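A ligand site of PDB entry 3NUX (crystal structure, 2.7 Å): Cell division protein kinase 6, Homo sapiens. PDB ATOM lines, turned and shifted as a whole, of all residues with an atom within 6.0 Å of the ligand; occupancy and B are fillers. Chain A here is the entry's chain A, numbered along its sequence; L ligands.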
ATOM      1  N   GLU A  18     -32.335  14.033  20.475  1.00  0.00           N
ATOM      2  CA  GLU A  18     -31.388  14.255  19.393  1.00  0.00           C
ATOM      3  C   GLU A  18     -30.018  13.755  19.837  1.00  0.00           C
ATOM      4  O   GLU A  18     -29.364  14.365  20.675  1.00  0.00           O
ATOM      5  CB  GLU A  18     -31.287  15.733  19.033  1.00  0.00           C
ATOM      6  CG  GLU A  18     -30.630  15.982  17.684  1.00  0.00           C
ATOM      7  CD  GLU A  18     -30.213  17.427  17.494  1.00  0.00           C
ATOM      8  OE1 GLU A  18     -30.202  17.885  16.327  1.00  0.00           O
ATOM      9  OE2 GLU A  18     -29.899  18.100  18.493  1.00  0.00           O
ATOM     10  N   ILE A  19     -29.618  12.635  19.256  1.00  0.00           N
ATOM     11  CA  ILE A  19     -28.353  11.979  19.552  1.00  0.00           C
ATOM     12  C   ILE A  19     -27.178  12.815  19.099  1.00  0.00           C
ATOM     13  O   ILE A  19     -26.321  13.203  19.893  1.00  0.00           O
ATOM     14  CB  ILE A  19     -28.296  10.592  18.857  1.00  0.00           C
ATOM     15  CG1 ILE A  19     -29.237   9.613  19.550  1.00  0.00           C
ATOM     16  CG2 ILE A  19     -26.890  10.067  18.880  1.00  0.00           C
ATOM     17  CD1 ILE A  19     -29.243   8.247  18.907  1.00  0.00           C
ATOM     18  N   GLY A  20     -27.138  13.085  17.803  1.00  0.00           N
ATOM     19  CA  GLY A  20     -26.057  13.871  17.265  1.00  0.00           C
ATOM     20  C   GLY A  20     -26.489  14.548  15.981  1.00  0.00           C
ATOM     21  O   GLY A  20     -27.539  14.225  15.413  1.00  0.00           O
ATOM     22  N   VAL A  27     -29.243  12.955  13.458  1.00  0.00           N
ATOM     23  CA  VAL A  27     -29.642  11.667  14.041  1.00  0.00           C
ATOM     24  C   VAL A  27     -30.400  11.761  15.360  1.00  0.00           C
ATOM     25  O   VAL A  27     -30.031  12.530  16.246  1.00  0.00           O
ATOM     26  CB  VAL A  27     -28.413  10.798  14.334  1.00  0.00           C
ATOM     27  CG1 VAL A  27     -28.852   9.418  14.780  1.00  0.00           C
ATOM     28  CG2 VAL A  27     -27.533  10.736  13.112  1.00  0.00           C
ATOM     29  N   ALA A  41     -32.238   4.329  16.155  1.00  0.00           N
ATOM     30  CA  ALA A  41     -31.560   5.544  15.761  1.00  0.00           C
ATOM     31  C   ALA A  41     -32.022   5.922  14.384  1.00  0.00           C
ATOM     32  O   ALA A  41     -31.762   5.222  13.424  1.00  0.00           O
ATOM     33  CB  ALA A  41     -30.075   5.322  15.766  1.00  0.00           C
ATOM     34  N   LEU A  42     -32.750   7.043  14.304  1.00  0.00           N
ATOM     35  CA  LEU A  42     -33.248   7.537  13.036  1.00  0.00           C
ATOM     36  C   LEU A  42     -32.328   8.603  12.471  1.00  0.00           C
ATOM     37  O   LEU A  42     -31.961   9.559  13.146  1.00  0.00           O
ATOM     38  CB  LEU A  42     -34.649   8.125  13.194  1.00  0.00           C
ATOM     39  CG  LEU A  42     -35.781   7.209  13.634  1.00  0.00           C
ATOM     40  CD1 LEU A  42     -37.089   7.811  13.143  1.00  0.00           C
ATOM     41  CD2 LEU A  42     -35.610   5.825  13.034  1.00  0.00           C
ATOM     42  N   LYS A  43     -31.937   8.413  11.216  1.00  0.00           N
ATOM     43  CA  LYS A  43     -31.077   9.369  10.547  1.00  0.00           C
ATOM     44  C   LYS A  43     -31.865   9.852   9.346  1.00  0.00           C
ATOM     45  O   LYS A  43     -32.304   9.063   8.509  1.00  0.00           O
ATOM     46  CB  LYS A  43     -29.754   8.700  10.120  1.00  0.00           C
ATOM     47  CG  LYS A  43     -28.786   9.640   9.418  1.00  0.00           C
ATOM     48  CD  LYS A  43     -27.349   9.466   9.904  1.00  0.00           C
ATOM     49  CE  LYS A  43     -26.826   8.080   9.602  1.00  0.00           C
ATOM     50  NZ  LYS A  43     -25.381   7.946   9.908  1.00  0.00           N
ATOM     51  N   VAL A  77     -23.530  -1.661  13.321  1.00  0.00           N
ATOM     52  CA  VAL A  77     -24.912  -1.466  13.748  1.00  0.00           C
ATOM     53  C   VAL A  77     -25.933  -2.035  12.764  1.00  0.00           C
ATOM     54  O   VAL A  77     -25.838  -1.816  11.565  1.00  0.00           O
ATOM     55  CB  VAL A  77     -25.237   0.036  13.977  1.00  0.00           C
ATOM     56  CG1 VAL A  77     -24.621   0.504  15.277  1.00  0.00           C
ATOM     57  CG2 VAL A  77     -24.708   0.854  12.834  1.00  0.00           C
ATOM     58  N   PHE A  98     -31.637   2.521  12.345  1.00  0.00           N
ATOM     59  CA  PHE A  98     -30.607   1.614  12.844  1.00  0.00           C
ATOM     60  C   PHE A  98     -30.882   1.230  14.284  1.00  0.00           C
ATOM     61  O   PHE A  98     -31.604   1.920  14.992  1.00  0.00           O
ATOM     62  CB  PHE A  98     -29.243   2.287  12.818  1.00  0.00           C
ATOM     63  CG  PHE A  98     -28.779   2.707  11.466  1.00  0.00           C
ATOM     64  CD1 PHE A  98     -27.965   1.869  10.713  1.00  0.00           C
ATOM     65  CD2 PHE A  98     -29.093   3.963  10.977  1.00  0.00           C
ATOM     66  CE1 PHE A  98     -27.451   2.291   9.518  1.00  0.00           C
ATOM     67  CE2 PHE A  98     -28.580   4.405   9.780  1.00  0.00           C
ATOM     68  CZ  PHE A  98     -27.751   3.569   9.043  1.00  0.00           C
ATOM     69  N   GLU A  99     -30.296   0.126  14.727  1.00  0.00           N
ATOM     70  CA  GLU A  99     -30.483  -0.277  16.104  1.00  0.00           C
ATOM     71  C   GLU A  99     -29.816   0.776  16.958  1.00  0.00           C
ATOM     72  O   GLU A  99     -28.829   1.374  16.544  1.00  0.00           O
ATOM     73  CB  GLU A  99     -29.832  -1.631  16.358  1.00  0.00           C
ATOM     74  CG  GLU A  99     -28.369  -1.673  16.060  1.00  0.00           C
ATOM     75  CD  GLU A  99     -27.735  -2.940  16.581  1.00  0.00           C
ATOM     76  OE1 GLU A  99     -26.816  -3.466  15.915  1.00  0.00           O
ATOM     77  OE2 GLU A  99     -28.149  -3.405  17.654  1.00  0.00           O
ATOM     78  N   HIS A 100     -30.340   0.996  18.164  1.00  0.00           N
ATOM     79  CA  HIS A 100     -29.788   1.988  19.086  1.00  0.00           C
ATOM     80  C   HIS A 100     -28.835   1.341  20.099  1.00  0.00           C
ATOM     81  O   HIS A 100     -29.084   0.245  20.580  1.00  0.00           O
ATOM     82  CB  HIS A 100     -30.945   2.676  19.817  1.00  0.00           C
ATOM     83  CG  HIS A 100     -30.517   3.688  20.843  1.00  0.00           C
ATOM     84  ND1 HIS A 100     -30.548   5.046  20.611  1.00  0.00           N
ATOM     85  CD2 HIS A 100     -30.013   3.523  22.087  1.00  0.00           C
ATOM     86  CE1 HIS A 100     -30.084   5.671  21.677  1.00  0.00           C
ATOM     87  NE2 HIS A 100     -29.754   4.773  22.582  1.00  0.00           N
ATOM     88  N   VAL A 101     -27.743   2.032  20.411  1.00  0.00           N
ATOM     89  CA  VAL A 101     -26.786   1.554  21.407  1.00  0.00           C
ATOM     90  C   VAL A 101     -26.734   2.658  22.452  1.00  0.00           C
ATOM     91  O   VAL A 101     -26.596   3.818  22.120  1.00  0.00           O
ATOM     92  CB  VAL A 101     -25.384   1.370  20.806  1.00  0.00           C
ATOM     93  CG1 VAL A 101     -24.418   0.877  21.870  1.00  0.00           C
ATOM     94  CG2 VAL A 101     -25.435   0.411  19.670  1.00  0.00           C
ATOM     95  N   ASP A 102     -26.854   2.301  23.723  1.00  0.00           N
ATOM     96  CA  ASP A 102     -26.851   3.302  24.776  1.00  0.00           C
ATOM     97  C   ASP A 102     -25.679   4.280  24.806  1.00  0.00           C
ATOM     98  O   ASP A 102     -25.867   5.461  25.078  1.00  0.00           O
ATOM     99  CB  ASP A 102     -26.967   2.611  26.138  1.00  0.00           C
ATOM    100  CG  ASP A 102     -28.370   2.134  26.439  1.00  0.00           C
ATOM    101  OD1 ASP A 102     -28.593   1.580  27.533  1.00  0.00           O
ATOM    102  OD2 ASP A 102     -29.270   2.322  25.582  1.00  0.00           O
ATOM    103  N   GLN A 103     -24.472   3.815  24.540  1.00  0.00           N
ATOM    104  CA  GLN A 103     -23.335   4.722  24.592  1.00  0.00           C
ATOM    105  C   GLN A 103     -22.238   4.453  23.554  1.00  0.00           C
ATOM    106  O   GLN A 103     -22.224   3.419  22.903  1.00  0.00           O
ATOM    107  CB  GLN A 103     -22.727   4.664  25.997  1.00  0.00           C
ATOM    108  CG  GLN A 103     -22.012   3.379  26.325  1.00  0.00           C
ATOM    109  CD  GLN A 103     -21.413   3.379  27.713  1.00  0.00           C
ATOM    110  OE1 GLN A 103     -20.699   2.458  28.087  1.00  0.00           O
ATOM    111  NE2 GLN A 103     -21.706   4.417  28.486  1.00  0.00           N
ATOM    112  N   ASP A 104     -21.325   5.426  23.415  1.00  0.00           N
ATOM    113  CA  ASP A 104     -20.181   5.328  22.504  1.00  0.00           C
ATOM    114  C   ASP A 104     -18.884   5.095  23.272  1.00  0.00           C
ATOM    115  O   ASP A 104     -18.869   5.115  24.501  1.00  0.00           O
ATOM    116  CB  ASP A 104     -20.050   6.594  21.632  1.00  0.00           C
ATOM    117  CG  ASP A 104     -19.837   7.870  22.429  1.00  0.00           C
ATOM    118  OD1 ASP A 104     -19.373   7.819  23.580  1.00  0.00           O
ATOM    119  OD2 ASP A 104     -20.137   8.943  21.879  1.00  0.00           O
ATOM    120  N   THR A 107     -17.901   8.028  25.935  1.00  0.00           N
ATOM    121  CA  THR A 107     -18.640   7.978  27.170  1.00  0.00           C
ATOM    122  C   THR A 107     -18.094   6.816  28.006  1.00  0.00           C
ATOM    123  O   THR A 107     -17.876   6.955  29.207  1.00  0.00           O
ATOM    124  CB  THR A 107     -20.126   7.759  26.876  1.00  0.00           C
ATOM    125  OG1 THR A 107     -20.572   8.771  25.976  1.00  0.00           O
ATOM    126  CG2 THR A 107     -20.940   7.808  28.154  1.00  0.00           C
ATOM    127  N   GLN A 149     -16.309   8.554  18.897  1.00  0.00           N
ATOM    128  CA  GLN A 149     -17.678   9.039  18.837  1.00  0.00           C
ATOM    129  C   GLN A 149     -18.576   8.222  17.952  1.00  0.00           C
ATOM    130  O   GLN A 149     -19.807   8.325  18.066  1.00  0.00           O
ATOM    131  CB  GLN A 149     -17.722  10.503  18.383  1.00  0.00           C
ATOM    132  CG  GLN A 149     -17.129  11.489  19.341  1.00  0.00           C
ATOM    133  CD  GLN A 149     -15.625  11.421  19.379  1.00  0.00           C
ATOM    134  OE1 GLN A 149     -15.008  10.738  18.547  1.00  0.00           O
ATOM    135  NE2 GLN A 149     -15.017  12.126  20.324  1.00  0.00           N
ATOM    136  N   ASN A 150     -18.020   7.421  17.050  1.00  0.00           N
ATOM    137  CA  ASN A 150     -18.894   6.599  16.217  1.00  0.00           C
ATOM    138  C   ASN A 150     -18.600   5.107  16.337  1.00  0.00           C
ATOM    139  O   ASN A 150     -18.916   4.301  15.460  1.00  0.00           O
ATOM    140  CB  ASN A 150     -18.883   7.067  14.752  1.00  0.00           C
ATOM    141  CG  ASN A 150     -17.500   7.318  14.231  1.00  0.00           C
ATOM    142  OD1 ASN A 150     -16.610   6.493  14.388  1.00  0.00           O
ATOM    143  ND2 ASN A 150     -17.314   8.461  13.587  1.00  0.00           N
ATOM    144  N   ILE A 151     -17.973   4.770  17.453  1.00  0.00           N
ATOM    145  CA  ILE A 151     -17.671   3.394  17.794  1.00  0.00           C
ATOM    146  C   ILE A 151     -18.584   3.183  19.016  1.00  0.00           C
ATOM    147  O   ILE A 151     -18.308   3.708  20.094  1.00  0.00           O
ATOM    148  CB  ILE A 151     -16.224   3.237  18.219  1.00  0.00           C
ATOM    149  CG1 ILE A 151     -15.305   3.318  17.005  1.00  0.00           C
ATOM    150  CG2 ILE A 151     -16.049   1.927  18.927  1.00  0.00           C
ATOM    151  CD1 ILE A 151     -13.853   3.148  17.358  1.00  0.00           C
ATOM    152  N   LEU A 152     -19.668   2.451  18.837  1.00  0.00           N
ATOM    153  CA  LEU A 152     -20.619   2.240  19.929  1.00  0.00           C
ATOM    154  C   LEU A 152     -20.379   0.992  20.774  1.00  0.00           C
ATOM    155  O   LEU A 152     -20.181  -0.095  20.245  1.00  0.00           O
ATOM    156  CB  LEU A 152     -22.026   2.190  19.378  1.00  0.00           C
ATOM    157  CG  LEU A 152     -22.307   3.208  18.283  1.00  0.00           C
ATOM    158  CD1 LEU A 152     -23.588   2.825  17.602  1.00  0.00           C
ATOM    159  CD2 LEU A 152     -22.387   4.606  18.862  1.00  0.00           C
ATOM    160  N   ALA A 162     -20.559   2.485  13.541  1.00  0.00           N
ATOM    161  CA  ALA A 162     -21.691   3.202  12.981  1.00  0.00           C
ATOM    162  C   ALA A 162     -21.193   4.424  12.223  1.00  0.00           C
ATOM    163  O   ALA A 162     -20.008   4.751  12.266  1.00  0.00           O
ATOM    164  CB  ALA A 162     -22.633   3.634  14.089  1.00  0.00           C
ATOM    165  N   ASP A 163     -22.096   5.083  11.515  1.00  0.00           N
ATOM    166  CA  ASP A 163     -21.765   6.319  10.803  1.00  0.00           C
ATOM    167  C   ASP A 163     -20.729   6.213   9.692  1.00  0.00           C
ATOM    168  O   ASP A 163     -19.739   6.938   9.689  1.00  0.00           O
ATOM    169  CB  ASP A 163     -21.309   7.353  11.837  1.00  0.00           C
ATOM    170  CG  ASP A 163     -21.676   8.774  11.459  1.00  0.00           C
ATOM    171  OD1 ASP A 163     -22.636   8.974  10.676  1.00  0.00           O
ATOM    172  OD2 ASP A 163     -21.013   9.705  11.966  1.00  0.00           O
HETATM  173  C1  LIG L   1     -23.118  11.098  22.128  1.00  0.00           C
HETATM  174  N1  LIG L   1     -24.401  10.382  22.355  1.00  0.00           N
HETATM  175 CL1  LIG L   1     -27.104   5.777  12.883  1.00  0.00          CL
HETATM  176  C2  LIG L   1     -22.394  11.494  23.469  1.00  0.00           C
HETATM  177  N2  LIG L   1     -23.271  12.362  24.273  1.00  0.00           N
HETATM  178  C3  LIG L   1     -24.485  11.588  24.645  1.00  0.00           C
HETATM  179  N3  LIG L   1     -26.418   7.396  21.279  1.00  0.00           N
HETATM  180  C4  LIG L   1     -25.257  11.064  23.377  1.00  0.00           C
HETATM  181  N4  LIG L   1     -26.084   5.732  19.782  1.00  0.00           N
HETATM  182  C5  LIG L   1     -26.018   8.543  21.937  1.00  0.00           C
HETATM  183  N5  LIG L   1     -25.309   7.705  13.139  1.00  0.00           N
HETATM  184  C6  LIG L   1     -24.776   9.225  21.685  1.00  0.00           C
HETATM  185  N6  LIG L   1     -24.472   8.335  13.968  1.00  0.00           N
HETATM  186  C7  LIG L   1     -23.921   8.597  20.714  1.00  0.00           C
HETATM  187  N7  LIG L   1     -26.799   4.117  18.349  1.00  0.00           N
HETATM  188  C8  LIG L   1     -24.331   7.407  20.033  1.00  0.00           C
HETATM  189  N8  LIG L   1     -25.862   6.118  17.481  1.00  0.00           N
HETATM  190  C9  LIG L   1     -25.596   6.829  20.356  1.00  0.00           C
HETATM  191  C10 LIG L   1     -25.586   6.642  15.088  1.00  0.00           C
HETATM  192  C11 LIG L   1     -25.971   6.697  13.775  1.00  0.00           C
HETATM  193  C12 LIG L   1     -24.601   7.721  15.141  1.00  0.00           C
HETATM  194  C13 LIG L   1     -23.754   8.261  16.286  1.00  0.00           C
HETATM  195  C14 LIG L   1     -22.331   7.682  16.243  1.00  0.00           C
HETATM  196  C15 LIG L   1     -23.726   9.795  16.238  1.00  0.00           C
HETATM  197  C16 LIG L   1     -26.044   5.694  16.178  1.00  0.00           C
HETATM  198  C17 LIG L   1     -26.618   4.424  15.942  1.00  0.00           C
HETATM  199  C18 LIG L   1     -26.994   3.684  17.084  1.00  0.00           C
HETATM  200  C19 LIG L   1     -26.273   5.319  18.497  1.00  0.00           C
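The backbone NH of Val 101 sits at hydrogen-bond distance from a nitrogen (N7) of the ligand, 3.1 Å away. The side-chain amino group (NZ) of Lys 43 lies close to a nitrogen (N5) of the ligand, at 3.2 Å. A nitrogen (N4) of the ligand lies close to the backbone carbonyl oxygen (O) of Val 101 (3.1 Å).
N of Val 27 sits at hydrogen-bond distance from O of Gly 20 (2.9 Å). N of Thr 107 sits at hydrogen-bond distance from OD1 of Asp 104 (2.8 Å). The backbone carbonyl oxygen (O) of Asn 150 is in hydrogen-bond range of the backbone NH (N) of Ala 162 (3.1 Å). The side-chain carboxylate of Asp 163 is in salt-bridge range of the side-chain amino group of Lys 43 (3.0 Å). N of Ala 41 is in hydrogen-bond range of O of Phe 98 (2.7 Å). The backbone NH (N) of Ile 19 lies within hydrogen-bond range of the backbone carbonyl oxygen (O) of Val 27 (3.0 Å).
Merely in contact with the ligand: Glu 99 (3.0 Å), Gln 149 (3.2 Å), Phe 98 (3.3 Å), Ile 19 (3.5 Å), Leu 152 (3.5 Å), Ala 41 (3.6 Å), Asn 150 (3.6 Å), Asp 104 (3.7 Å), His 100 (3.7 Å), Val 27 (3.8 Å) and Asp 163 (3.8 Å). Hydrophobic or aromatic side chains that line the ligand: Ile 19, Val 27, Ala 41, Phe 98, Val 101 and Leu 152. 13 residues have an atom within 4 Å of the ligand: Ile 19, Val 27, Ala 41, Lys 43, Phe 98, Glu 99, His 100, Val 101, Asp 104, Gln 149, Asn 150, Leu 152 and Asp 163.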
